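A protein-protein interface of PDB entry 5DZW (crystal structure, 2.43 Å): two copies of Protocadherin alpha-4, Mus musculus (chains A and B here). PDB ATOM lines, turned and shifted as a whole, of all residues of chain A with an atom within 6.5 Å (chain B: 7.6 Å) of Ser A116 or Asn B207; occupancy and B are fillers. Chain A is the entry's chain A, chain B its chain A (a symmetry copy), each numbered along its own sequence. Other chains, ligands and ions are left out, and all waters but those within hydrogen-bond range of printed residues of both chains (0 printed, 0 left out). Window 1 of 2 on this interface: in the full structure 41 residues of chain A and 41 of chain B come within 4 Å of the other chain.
Among the printed residues, merely in contact across the chains: Leu A299 with Ser B116, Ser A116 with Leu B299, Pro A118 with Asp B208, Arg A117 with Leu B301, Ala A206 with Leu B299, Leu A299 with Ala B206, Ala A114 with Leu B299, Ser A116 with Leu B301, Ser A116 with Asn B207, Leu A204 with Leu B299 and Leu A299 with Leu B204.
Asn B207 touches just one residue of chain A: Ser A116. Printed residues of chain A within 4 Å of Ala B206: Leu A299 (3.6 Å). Printed residues of chain B within 4 Å of Ala A114: Leu B299 (3.7 Å).
N of Leu A204 is in hydrogen-bond range of O of Ile A113. The backbone NH (N) of Ala A206 lies within hydrogen-bond range of the side-chain carboxylate (OE1) of Glu A115 (3.1 Å). The backbone NH of Glu B115 lies close to the backbone carbonyl oxygen of Leu B204, at 3.4 Å. The backbone NH (N) of Ala B206 is in hydrogen-bond range of the side-chain carboxylate (OE1) of Glu B115 (3.1 Å). O of Leu B299 sits at hydrogen-bond distance from ND2 of Asn B207 (2.6 Å). OD1 of Asp B295 sits at hydrogen-bond distance from N of Leu B301 (2.6 Å).
Hydrophobic or aromatic side chains of chain A that line the printed part of chain B: Ala A114, Pro A118, Leu A204, Ala A206 and Leu A299. Of the 24 printed residues of chain B, 7 touch a printed residue of chain A. Hydrophobic or aromatic side chains of chain B that line the printed part of chain A: Leu B204, Ala B206, Leu B299 and Leu B301. Among the printed residues, 11 pairs touch across the chains.
Ser A116 touches Leu B299, and with the chains exchanged Leu A299 touches Ser B116. Leu A204 touches Leu B299, and with the chains exchanged Leu A299 touches Leu B204. Ala A206 touches Leu B299, and with the chains exchanged Leu A299 touches Ala B206. Of the 11 pairs that touch across the chains among the printed residues, 6 have their exchanged pair printed and touching as well.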
ATOM      1  N   ILE A 113       2.311  19.528 -36.625  1.00  0.00           N
ATOM      2  CA  ILE A 113       3.152  18.799 -35.684  1.00  0.00           C
ATOM      3  C   ILE A 113       4.515  19.468 -35.525  1.00  0.00           C
ATOM      4  O   ILE A 113       5.178  19.791 -36.511  1.00  0.00           O
ATOM      5  CB  ILE A 113       3.334  17.339 -36.137  1.00  0.00           C
ATOM      6  CG1 ILE A 113       1.978  16.635 -36.180  1.00  0.00           C
ATOM      7  CG2 ILE A 113       4.292  16.601 -35.221  1.00  0.00           C
ATOM      8  CD1 ILE A 113       2.042  15.211 -36.661  1.00  0.00           C
ATOM      9  N   ALA A 114       4.927  19.676 -34.278  1.00  0.00           N
ATOM     10  CA  ALA A 114       6.163  20.393 -33.978  1.00  0.00           C
ATOM     11  C   ALA A 114       7.409  19.574 -34.309  1.00  0.00           C
ATOM     12  O   ALA A 114       7.407  18.348 -34.206  1.00  0.00           O
ATOM     13  CB  ALA A 114       6.184  20.806 -32.516  1.00  0.00           C
ATOM     14  N   GLU A 115       8.472  20.269 -34.701  1.00  0.00           N
ATOM     15  CA  GLU A 115       9.743  19.632 -35.026  1.00  0.00           C
ATOM     16  C   GLU A 115      10.442  19.139 -33.762  1.00  0.00           C
ATOM     17  O   GLU A 115      11.301  18.258 -33.814  1.00  0.00           O
ATOM     18  CB  GLU A 115      10.644  20.610 -35.784  1.00  0.00           C
ATOM     19  CG  GLU A 115      11.941  20.018 -36.298  1.00  0.00           C
ATOM     20  CD  GLU A 115      12.900  21.078 -36.802  1.00  0.00           C
ATOM     21  OE1 GLU A 115      12.522  22.269 -36.808  1.00  0.00           O
ATOM     22  OE2 GLU A 115      14.032  20.720 -37.186  1.00  0.00           O
ATOM     23  N   SER A 116      10.060  19.709 -32.625  1.00  0.00           N
ATOM     24  CA  SER A 116      10.695  19.384 -31.355  1.00  0.00           C
ATOM     25  C   SER A 116      10.033  18.207 -30.645  1.00  0.00           C
ATOM     26  O   SER A 116      10.489  17.790 -29.581  1.00  0.00           O
ATOM     27  CB  SER A 116      10.684  20.607 -30.435  1.00  0.00           C
ATOM     28  OG  SER A 116       9.359  21.018 -30.151  1.00  0.00           O
ATOM     29  N   ARG A 117       8.962  17.674 -31.232  1.00  0.00           N
ATOM     30  CA  ARG A 117       8.211  16.585 -30.607  1.00  0.00           C
ATOM     31  C   ARG A 117       9.057  15.326 -30.435  1.00  0.00           C
ATOM     32  O   ARG A 117       9.690  14.862 -31.385  1.00  0.00           O
ATOM     33  CB  ARG A 117       6.953  16.257 -31.416  1.00  0.00           C
ATOM     34  CG  ARG A 117       5.864  17.311 -31.326  1.00  0.00           C
ATOM     35  CD  ARG A 117       4.499  16.743 -31.691  1.00  0.00           C
ATOM     36  NE  ARG A 117       3.464  17.772 -31.689  1.00  0.00           N
ATOM     37  CZ  ARG A 117       2.700  18.060 -30.640  1.00  0.00           C
ATOM     38  NH1 ARG A 117       2.848  17.393 -29.505  1.00  0.00           N
ATOM     39  NH2 ARG A 117       1.784  19.016 -30.730  1.00  0.00           N
ATOM     40  N   PRO A 118       9.067  14.775 -29.212  1.00  0.00           N
ATOM     41  CA  PRO A 118       9.831  13.573 -28.855  1.00  0.00           C
ATOM     42  C   PRO A 118       9.391  12.342 -29.639  1.00  0.00           C
ATOM     43  O   PRO A 118       8.267  12.294 -30.137  1.00  0.00           O
ATOM     44  CB  PRO A 118       9.531  13.395 -27.361  1.00  0.00           C
ATOM     45  CG  PRO A 118       9.082  14.738 -26.891  1.00  0.00           C
ATOM     46  CD  PRO A 118       8.359  15.341 -28.051  1.00  0.00           C
ATOM     47  N   LEU A 119      10.277  11.355 -29.741  1.00  0.00           N
ATOM     48  CA  LEU A 119       9.951  10.102 -30.409  1.00  0.00           C
ATOM     49  C   LEU A 119       9.022   9.261 -29.541  1.00  0.00           C
ATOM     50  O   LEU A 119       8.883   9.519 -28.343  1.00  0.00           O
ATOM     51  CB  LEU A 119      11.224   9.321 -30.738  1.00  0.00           C
ATOM     52  CG  LEU A 119      12.182   9.985 -31.730  1.00  0.00           C
ATOM     53  CD1 LEU A 119      13.457   9.168 -31.882  1.00  0.00           C
ATOM     54  CD2 LEU A 119      11.501  10.176 -33.077  1.00  0.00           C
ATOM     55  N   LEU A 171      12.381  14.217 -37.077  1.00  0.00           N
ATOM     56  CA  LEU A 171      11.794  15.099 -38.079  1.00  0.00           C
ATOM     57  C   LEU A 171      12.518  16.441 -38.132  1.00  0.00           C
ATOM     58  O   LEU A 171      12.880  17.006 -37.100  1.00  0.00           O
ATOM     59  CB  LEU A 171      10.300  15.312 -37.803  1.00  0.00           C
ATOM     60  CG  LEU A 171       9.845  16.190 -36.631  1.00  0.00           C
ATOM     61  CD1 LEU A 171       8.355  16.479 -36.745  1.00  0.00           C
ATOM     62  CD2 LEU A 171      10.168  15.566 -35.279  1.00  0.00           C
ATOM     63  N   VAL A 203       5.264  20.433 -40.719  1.00  0.00           N
ATOM     64  CA  VAL A 203       6.122  20.448 -39.539  1.00  0.00           C
ATOM     65  C   VAL A 203       6.489  21.880 -39.151  1.00  0.00           C
ATOM     66  O   VAL A 203       6.920  22.675 -39.986  1.00  0.00           O
ATOM     67  CB  VAL A 203       7.404  19.611 -39.757  1.00  0.00           C
ATOM     68  CG1 VAL A 203       8.078  19.981 -41.065  1.00  0.00           C
ATOM     69  CG2 VAL A 203       8.362  19.778 -38.588  1.00  0.00           C
ATOM     70  N   LEU A 204       6.292  22.204 -37.878  1.00  0.00           N
ATOM     71  CA  LEU A 204       6.516  23.555 -37.382  1.00  0.00           C
ATOM     72  C   LEU A 204       8.002  23.820 -37.156  1.00  0.00           C
ATOM     73  O   LEU A 204       8.766  22.902 -36.861  1.00  0.00           O
ATOM     74  CB  LEU A 204       5.726  23.782 -36.090  1.00  0.00           C
ATOM     75  CG  LEU A 204       4.235  23.434 -36.171  1.00  0.00           C
ATOM     76  CD1 LEU A 204       3.545  23.647 -34.832  1.00  0.00           C
ATOM     77  CD2 LEU A 204       3.547  24.238 -37.267  1.00  0.00           C
ATOM     78  N   ALA A 206      11.217  24.678 -35.358  1.00  0.00           N
ATOM     79  CA  ALA A 206      11.807  24.715 -34.027  1.00  0.00           C
ATOM     80  C   ALA A 206      13.138  25.456 -34.066  1.00  0.00           C
ATOM     81  O   ALA A 206      13.769  25.550 -35.117  1.00  0.00           O
ATOM     82  CB  ALA A 206      11.993  23.306 -33.486  1.00  0.00           C
ATOM     83  N   LEU A 299      14.825  30.113 -26.803  1.00  0.00           N
ATOM     84  CA  LEU A 299      16.109  29.600 -26.349  1.00  0.00           C
ATOM     85  C   LEU A 299      17.160  29.916 -27.403  1.00  0.00           C
ATOM     86  O   LEU A 299      17.312  29.175 -28.375  1.00  0.00           O
ATOM     87  CB  LEU A 299      16.044  28.095 -26.086  1.00  0.00           C
ATOM     88  CG  LEU A 299      17.343  27.460 -25.586  1.00  0.00           C
ATOM     89  CD1 LEU A 299      17.839  28.171 -24.338  1.00  0.00           C
ATOM     90  CD2 LEU A 299      17.149  25.978 -25.317  1.00  0.00           C
ATOM     91  N   GLU B 115      20.099  23.305 -24.092  1.00  0.00           N
ATOM     92  CA  GLU B 115      19.799  21.886 -24.243  1.00  0.00           C
ATOM     93  C   GLU B 115      19.493  21.547 -25.699  1.00  0.00           C
ATOM     94  O   GLU B 115      19.595  20.394 -26.118  1.00  0.00           O
ATOM     95  CB  GLU B 115      18.620  21.499 -23.349  1.00  0.00           C
ATOM     96  CG  GLU B 115      18.302  20.017 -23.314  1.00  0.00           C
ATOM     97  CD  GLU B 115      16.979  19.726 -22.633  1.00  0.00           C
ATOM     98  OE1 GLU B 115      16.345  20.679 -22.130  1.00  0.00           O
ATOM     99  OE2 GLU B 115      16.574  18.546 -22.604  1.00  0.00           O
ATOM    100  N   SER B 116      19.125  22.566 -26.469  1.00  0.00           N
ATOM    101  CA  SER B 116      18.735  22.372 -27.859  1.00  0.00           C
ATOM    102  C   SER B 116      19.915  22.452 -28.822  1.00  0.00           C
ATOM    103  O   SER B 116      19.745  22.264 -30.027  1.00  0.00           O
ATOM    104  CB  SER B 116      17.680  23.406 -28.256  1.00  0.00           C
ATOM    105  OG  SER B 116      18.189  24.723 -28.140  1.00  0.00           O
ATOM    106  N   GLU B 174      16.791  17.861 -17.746  1.00  0.00           N
ATOM    107  CA  GLU B 174      16.057  17.152 -16.701  1.00  0.00           C
ATOM    108  C   GLU B 174      16.882  16.033 -16.067  1.00  0.00           C
ATOM    109  O   GLU B 174      16.783  15.786 -14.866  1.00  0.00           O
ATOM    110  CB  GLU B 174      14.750  16.578 -17.259  1.00  0.00           C
ATOM    111  CG  GLU B 174      13.657  17.611 -17.490  1.00  0.00           C
ATOM    112  CD  GLU B 174      13.940  18.517 -18.673  1.00  0.00           C
ATOM    113  OE1 GLU B 174      14.758  18.130 -19.534  1.00  0.00           O
ATOM    114  OE2 GLU B 174      13.349  19.614 -18.738  1.00  0.00           O
ATOM    115  N   LEU B 204      20.630  24.863 -20.107  1.00  0.00           N
ATOM    116  CA  LEU B 204      19.400  25.643 -20.110  1.00  0.00           C
ATOM    117  C   LEU B 204      18.198  24.775 -20.476  1.00  0.00           C
ATOM    118  O   LEU B 204      18.330  23.797 -21.210  1.00  0.00           O
ATOM    119  CB  LEU B 204      19.525  26.824 -21.076  1.00  0.00           C
ATOM    120  CG  LEU B 204      20.766  27.701 -20.872  1.00  0.00           C
ATOM    121  CD1 LEU B 204      20.829  28.817 -21.904  1.00  0.00           C
ATOM    122  CD2 LEU B 204      20.807  28.267 -19.459  1.00  0.00           C
ATOM    123  N   ASP B 205      17.029  25.137 -19.958  1.00  0.00           N
ATOM    124  CA  ASP B 205      15.821  24.349 -20.176  1.00  0.00           C
ATOM    125  C   ASP B 205      15.224  24.591 -21.559  1.00  0.00           C
ATOM    126  O   ASP B 205      14.828  25.709 -21.889  1.00  0.00           O
ATOM    127  CB  ASP B 205      14.780  24.661 -19.098  1.00  0.00           C
ATOM    128  CG  ASP B 205      13.508  23.849 -19.262  1.00  0.00           C
ATOM    129  OD1 ASP B 205      13.596  22.671 -19.667  1.00  0.00           O
ATOM    130  OD2 ASP B 205      12.416  24.390 -18.984  1.00  0.00           O
ATOM    131  N   ALA B 206      15.164  23.534 -22.362  1.00  0.00           N
ATOM    132  CA  ALA B 206      14.525  23.602 -23.669  1.00  0.00           C
ATOM    133  C   ALA B 206      13.118  23.022 -23.592  1.00  0.00           C
ATOM    134  O   ALA B 206      12.818  22.227 -22.703  1.00  0.00           O
ATOM    135  CB  ALA B 206      15.353  22.862 -24.707  1.00  0.00           C
ATOM    136  N   ASN B 207      12.255  23.425 -24.519  1.00  0.00           N
ATOM    137  CA  ASN B 207      10.889  22.913 -24.548  1.00  0.00           C
ATOM    138  C   ASN B 207      10.791  21.656 -25.403  1.00  0.00           C
ATOM    139  O   ASN B 207      10.187  21.667 -26.476  1.00  0.00           O
ATOM    140  CB  ASN B 207       9.924  23.980 -25.068  1.00  0.00           C
ATOM    141  CG  ASN B 207       8.470  23.608 -24.847  1.00  0.00           C
ATOM    142  OD1 ASN B 207       8.142  22.851 -23.934  1.00  0.00           O
ATOM    143  ND2 ASN B 207       7.590  24.139 -25.689  1.00  0.00           N
ATOM    144  N   ASP B 208      11.389  20.570 -24.922  1.00  0.00           N
ATOM    145  CA  ASP B 208      11.457  19.333 -25.692  1.00  0.00           C
ATOM    146  C   ASP B 208      10.716  18.185 -25.015  1.00  0.00           C
ATOM    147  O   ASP B 208      10.874  17.025 -25.399  1.00  0.00           O
ATOM    148  CB  ASP B 208      12.916  18.940 -25.936  1.00  0.00           C
ATOM    149  CG  ASP B 208      13.714  18.827 -24.650  1.00  0.00           C
ATOM    150  OD1 ASP B 208      13.434  19.594 -23.705  1.00  0.00           O
ATOM    151  OD2 ASP B 208      14.624  17.972 -24.587  1.00  0.00           O
ATOM    152  N   ASN B 209       9.909  18.508 -24.010  1.00  0.00           N
ATOM    153  CA  ASN B 209       9.094  17.504 -23.336  1.00  0.00           C
ATOM    154  C   ASN B 209       7.615  17.878 -23.302  1.00  0.00           C
ATOM    155  O   ASN B 209       7.247  18.960 -22.848  1.00  0.00           O
ATOM    156  CB  ASN B 209       9.600  17.269 -21.911  1.00  0.00           C
ATOM    157  CG  ASN B 209      10.762  16.298 -21.858  1.00  0.00           C
ATOM    158  OD1 ASN B 209      11.586  16.247 -22.770  1.00  0.00           O
ATOM    159  ND2 ASN B 209      10.827  15.512 -20.791  1.00  0.00           N
ATOM    160  N   ALA B 210       6.776  16.969 -23.788  1.00  0.00           N
ATOM    161  CA  ALA B 210       5.334  17.183 -23.810  1.00  0.00           C
ATOM    162  C   ALA B 210       4.707  16.796 -22.474  1.00  0.00           C
ATOM    163  O   ALA B 210       5.216  15.917 -21.779  1.00  0.00           O
ATOM    164  CB  ALA B 210       4.700  16.388 -24.946  1.00  0.00           C
ATOM    165  N   PRO B 211       3.602  17.464 -22.105  1.00  0.00           N
ATOM    166  CA  PRO B 211       2.877  17.124 -20.874  1.00  0.00           C
ATOM    167  C   PRO B 211       2.296  15.714 -20.918  1.00  0.00           C
ATOM    168  O   PRO B 211       1.979  15.212 -21.996  1.00  0.00           O
ATOM    169  CB  PRO B 211       1.763  18.175 -20.818  1.00  0.00           C
ATOM    170  CG  PRO B 211       1.634  18.680 -22.211  1.00  0.00           C
ATOM    171  CD  PRO B 211       3.007  18.623 -22.790  1.00  0.00           C
ATOM    172  N   ASP B 239       4.510  17.847 -16.473  1.00  0.00           N
ATOM    173  CA  ASP B 239       5.496  18.143 -17.506  1.00  0.00           C
ATOM    174  C   ASP B 239       6.864  18.419 -16.886  1.00  0.00           C
ATOM    175  O   ASP B 239       6.971  19.128 -15.885  1.00  0.00           O
ATOM    176  CB  ASP B 239       5.041  19.334 -18.351  1.00  0.00           C
ATOM    177  CG  ASP B 239       5.906  19.545 -19.577  1.00  0.00           C
ATOM    178  OD1 ASP B 239       6.685  18.634 -19.930  1.00  0.00           O
ATOM    179  OD2 ASP B 239       5.798  20.623 -20.193  1.00  0.00           O
ATOM    180  N   ASP B 241       9.516  20.021 -18.083  1.00  0.00           N
ATOM    181  CA  ASP B 241      10.121  21.327 -18.323  1.00  0.00           C
ATOM    182  C   ASP B 241       9.686  22.333 -17.262  1.00  0.00           C
ATOM    183  O   ASP B 241       8.733  22.093 -16.520  1.00  0.00           O
ATOM    184  CB  ASP B 241       9.769  21.840 -19.720  1.00  0.00           C
ATOM    185  CG  ASP B 241      10.264  20.921 -20.818  1.00  0.00           C
ATOM    186  OD1 ASP B 241      10.954  19.929 -20.501  1.00  0.00           O
ATOM    187  OD2 ASP B 241       9.970  21.192 -22.000  1.00  0.00           O
ATOM    188  N   GLU B 242      10.392  23.458 -17.195  1.00  0.00           N
ATOM    189  CA  GLU B 242      10.125  24.471 -16.179  1.00  0.00           C
ATOM    190  C   GLU B 242       9.687  25.794 -16.798  1.00  0.00           C
ATOM    191  O   GLU B 242       9.810  25.998 -18.006  1.00  0.00           O
ATOM    192  CB  GLU B 242      11.362  24.686 -15.306  1.00  0.00           C
ATOM    193  N   VAL B 244       7.306  28.684 -18.263  1.00  0.00           N
ATOM    194  CA  VAL B 244       6.134  28.648 -19.131  1.00  0.00           C
ATOM    195  C   VAL B 244       6.125  27.368 -19.958  1.00  0.00           C
ATOM    196  O   VAL B 244       5.091  26.969 -20.490  1.00  0.00           O
ATOM    197  CB  VAL B 244       6.076  29.867 -20.073  1.00  0.00           C
ATOM    198  CG1 VAL B 244       5.904  31.150 -19.274  1.00  0.00           C
ATOM    199  CG2 VAL B 244       7.324  29.931 -20.942  1.00  0.00           C
ATOM    200  N   ASN B 245       7.284  26.723 -20.058  1.00  0.00           N
ATOM    201  CA  ASN B 245       7.391  25.450 -20.756  1.00  0.00           C
ATOM    202  C   ASN B 245       6.862  24.307 -19.898  1.00  0.00           C
ATOM    203  O   ASN B 245       6.720  23.181 -20.370  1.00  0.00           O
ATOM    204  CB  ASN B 245       8.842  25.182 -21.157  1.00  0.00           C
ATOM    205  CG  ASN B 245       9.380  26.218 -22.122  1.00  0.00           C
ATOM    206  OD1 ASN B 245       8.707  27.199 -22.438  1.00  0.00           O
ATOM    207  ND2 ASN B 245      10.606  26.012 -22.590  1.00  0.00           N
ATOM    208  N   GLY B 246       6.571  24.608 -18.637  1.00  0.00           N
ATOM    209  CA  GLY B 246       6.068  23.615 -17.706  1.00  0.00           C
ATOM    210  C   GLY B 246       4.592  23.774 -17.392  1.00  0.00           C
ATOM    211  O   GLY B 246       3.904  22.790 -17.123  1.00  0.00           O
ATOM    212  N   ASP B 295       1.294  22.981 -23.210  1.00  0.00           N
ATOM    213  CA  ASP B 295       2.143  23.878 -22.432  1.00  0.00           C
ATOM    214  C   ASP B 295       2.165  25.278 -23.038  1.00  0.00           C
ATOM    215  O   ASP B 295       1.535  25.529 -24.067  1.00  0.00           O
ATOM    216  CB  ASP B 295       3.565  23.318 -22.314  1.00  0.00           C
ATOM    217  CG  ASP B 295       4.102  22.792 -23.633  1.00  0.00           C
ATOM    218  OD1 ASP B 295       3.773  23.367 -24.690  1.00  0.00           O
ATOM    219  OD2 ASP B 295       4.858  21.796 -23.609  1.00  0.00           O
ATOM    220  N   LYS B 296       2.890  26.188 -22.395  1.00  0.00           N
ATOM    221  CA  LYS B 296       2.896  27.587 -22.810  1.00  0.00           C
ATOM    222  C   LYS B 296       4.268  28.046 -23.295  1.00  0.00           C
ATOM    223  O   LYS B 296       4.708  29.152 -22.982  1.00  0.00           O
ATOM    224  CB  LYS B 296       2.431  28.479 -21.655  1.00  0.00           C
ATOM    225  CG  LYS B 296       1.075  28.099 -21.084  1.00  0.00           C
ATOM    226  CD  LYS B 296       0.706  28.983 -19.905  1.00  0.00           C
ATOM    227  N   GLY B 297       4.940  27.194 -24.063  1.00  0.00           N
ATOM    228  CA  GLY B 297       6.244  27.531 -24.605  1.00  0.00           C
ATOM    229  C   GLY B 297       6.145  28.225 -25.949  1.00  0.00           C
ATOM    230  O   GLY B 297       5.047  28.416 -26.475  1.00  0.00           O
ATOM    231  N   GLN B 298       7.292  28.610 -26.502  1.00  0.00           N
ATOM    232  CA  GLN B 298       7.340  29.235 -27.820  1.00  0.00           C
ATOM    233  C   GLN B 298       6.823  28.274 -28.880  1.00  0.00           C
ATOM    234  O   GLN B 298       5.990  28.636 -29.711  1.00  0.00           O
ATOM    235  CB  GLN B 298       8.765  29.679 -28.158  1.00  0.00           C
ATOM    236  N   LEU B 299       7.330  27.047 -28.847  1.00  0.00           N
ATOM    237  CA  LEU B 299       6.797  25.971 -29.668  1.00  0.00           C
ATOM    238  C   LEU B 299       6.060  24.990 -28.768  1.00  0.00           C
ATOM    239  O   LEU B 299       6.675  24.105 -28.172  1.00  0.00           O
ATOM    240  CB  LEU B 299       7.908  25.261 -30.443  1.00  0.00           C
ATOM    241  CG  LEU B 299       7.447  24.121 -31.354  1.00  0.00           C
ATOM    242  CD1 LEU B 299       6.384  24.610 -32.325  1.00  0.00           C
ATOM    243  CD2 LEU B 299       8.624  23.523 -32.105  1.00  0.00           C
ATOM    244  N   PRO B 300       4.733  25.156 -28.659  1.00  0.00           N
ATOM    245  CA  PRO B 300       3.899  24.379 -27.735  1.00  0.00           C
ATOM    246  C   PRO B 300       3.897  22.883 -28.028  1.00  0.00           C
ATOM    247  O   PRO B 300       3.852  22.474 -29.189  1.00  0.00           O
ATOM    248  CB  PRO B 300       2.500  24.968 -27.948  1.00  0.00           C
ATOM    249  CG  PRO B 300       2.733  26.317 -28.541  1.00  0.00           C
ATOM    250  CD  PRO B 300       3.947  26.159 -29.395  1.00  0.00           C
ATOM    251  N   LEU B 301       3.953  22.080 -26.970  1.00  0.00           N
ATOM    252  CA  LEU B 301       3.796  20.636 -27.085  1.00  0.00           C
ATOM    253  C   LEU B 301       2.494  20.203 -26.420  1.00  0.00           C
ATOM    254  O   LEU B 301       2.088  20.771 -25.404  1.00  0.00           O
ATOM    255  CB  LEU B 301       4.986  19.906 -26.460  1.00  0.00           C
ATOM    256  CG  LEU B 301       6.323  20.054 -27.184  1.00  0.00           C
ATOM    257  CD1 LEU B 301       7.385  19.176 -26.540  1.00  0.00           C
ATOM    258  CD2 LEU B 301       6.169  19.721 -28.658  1.00  0.00           C
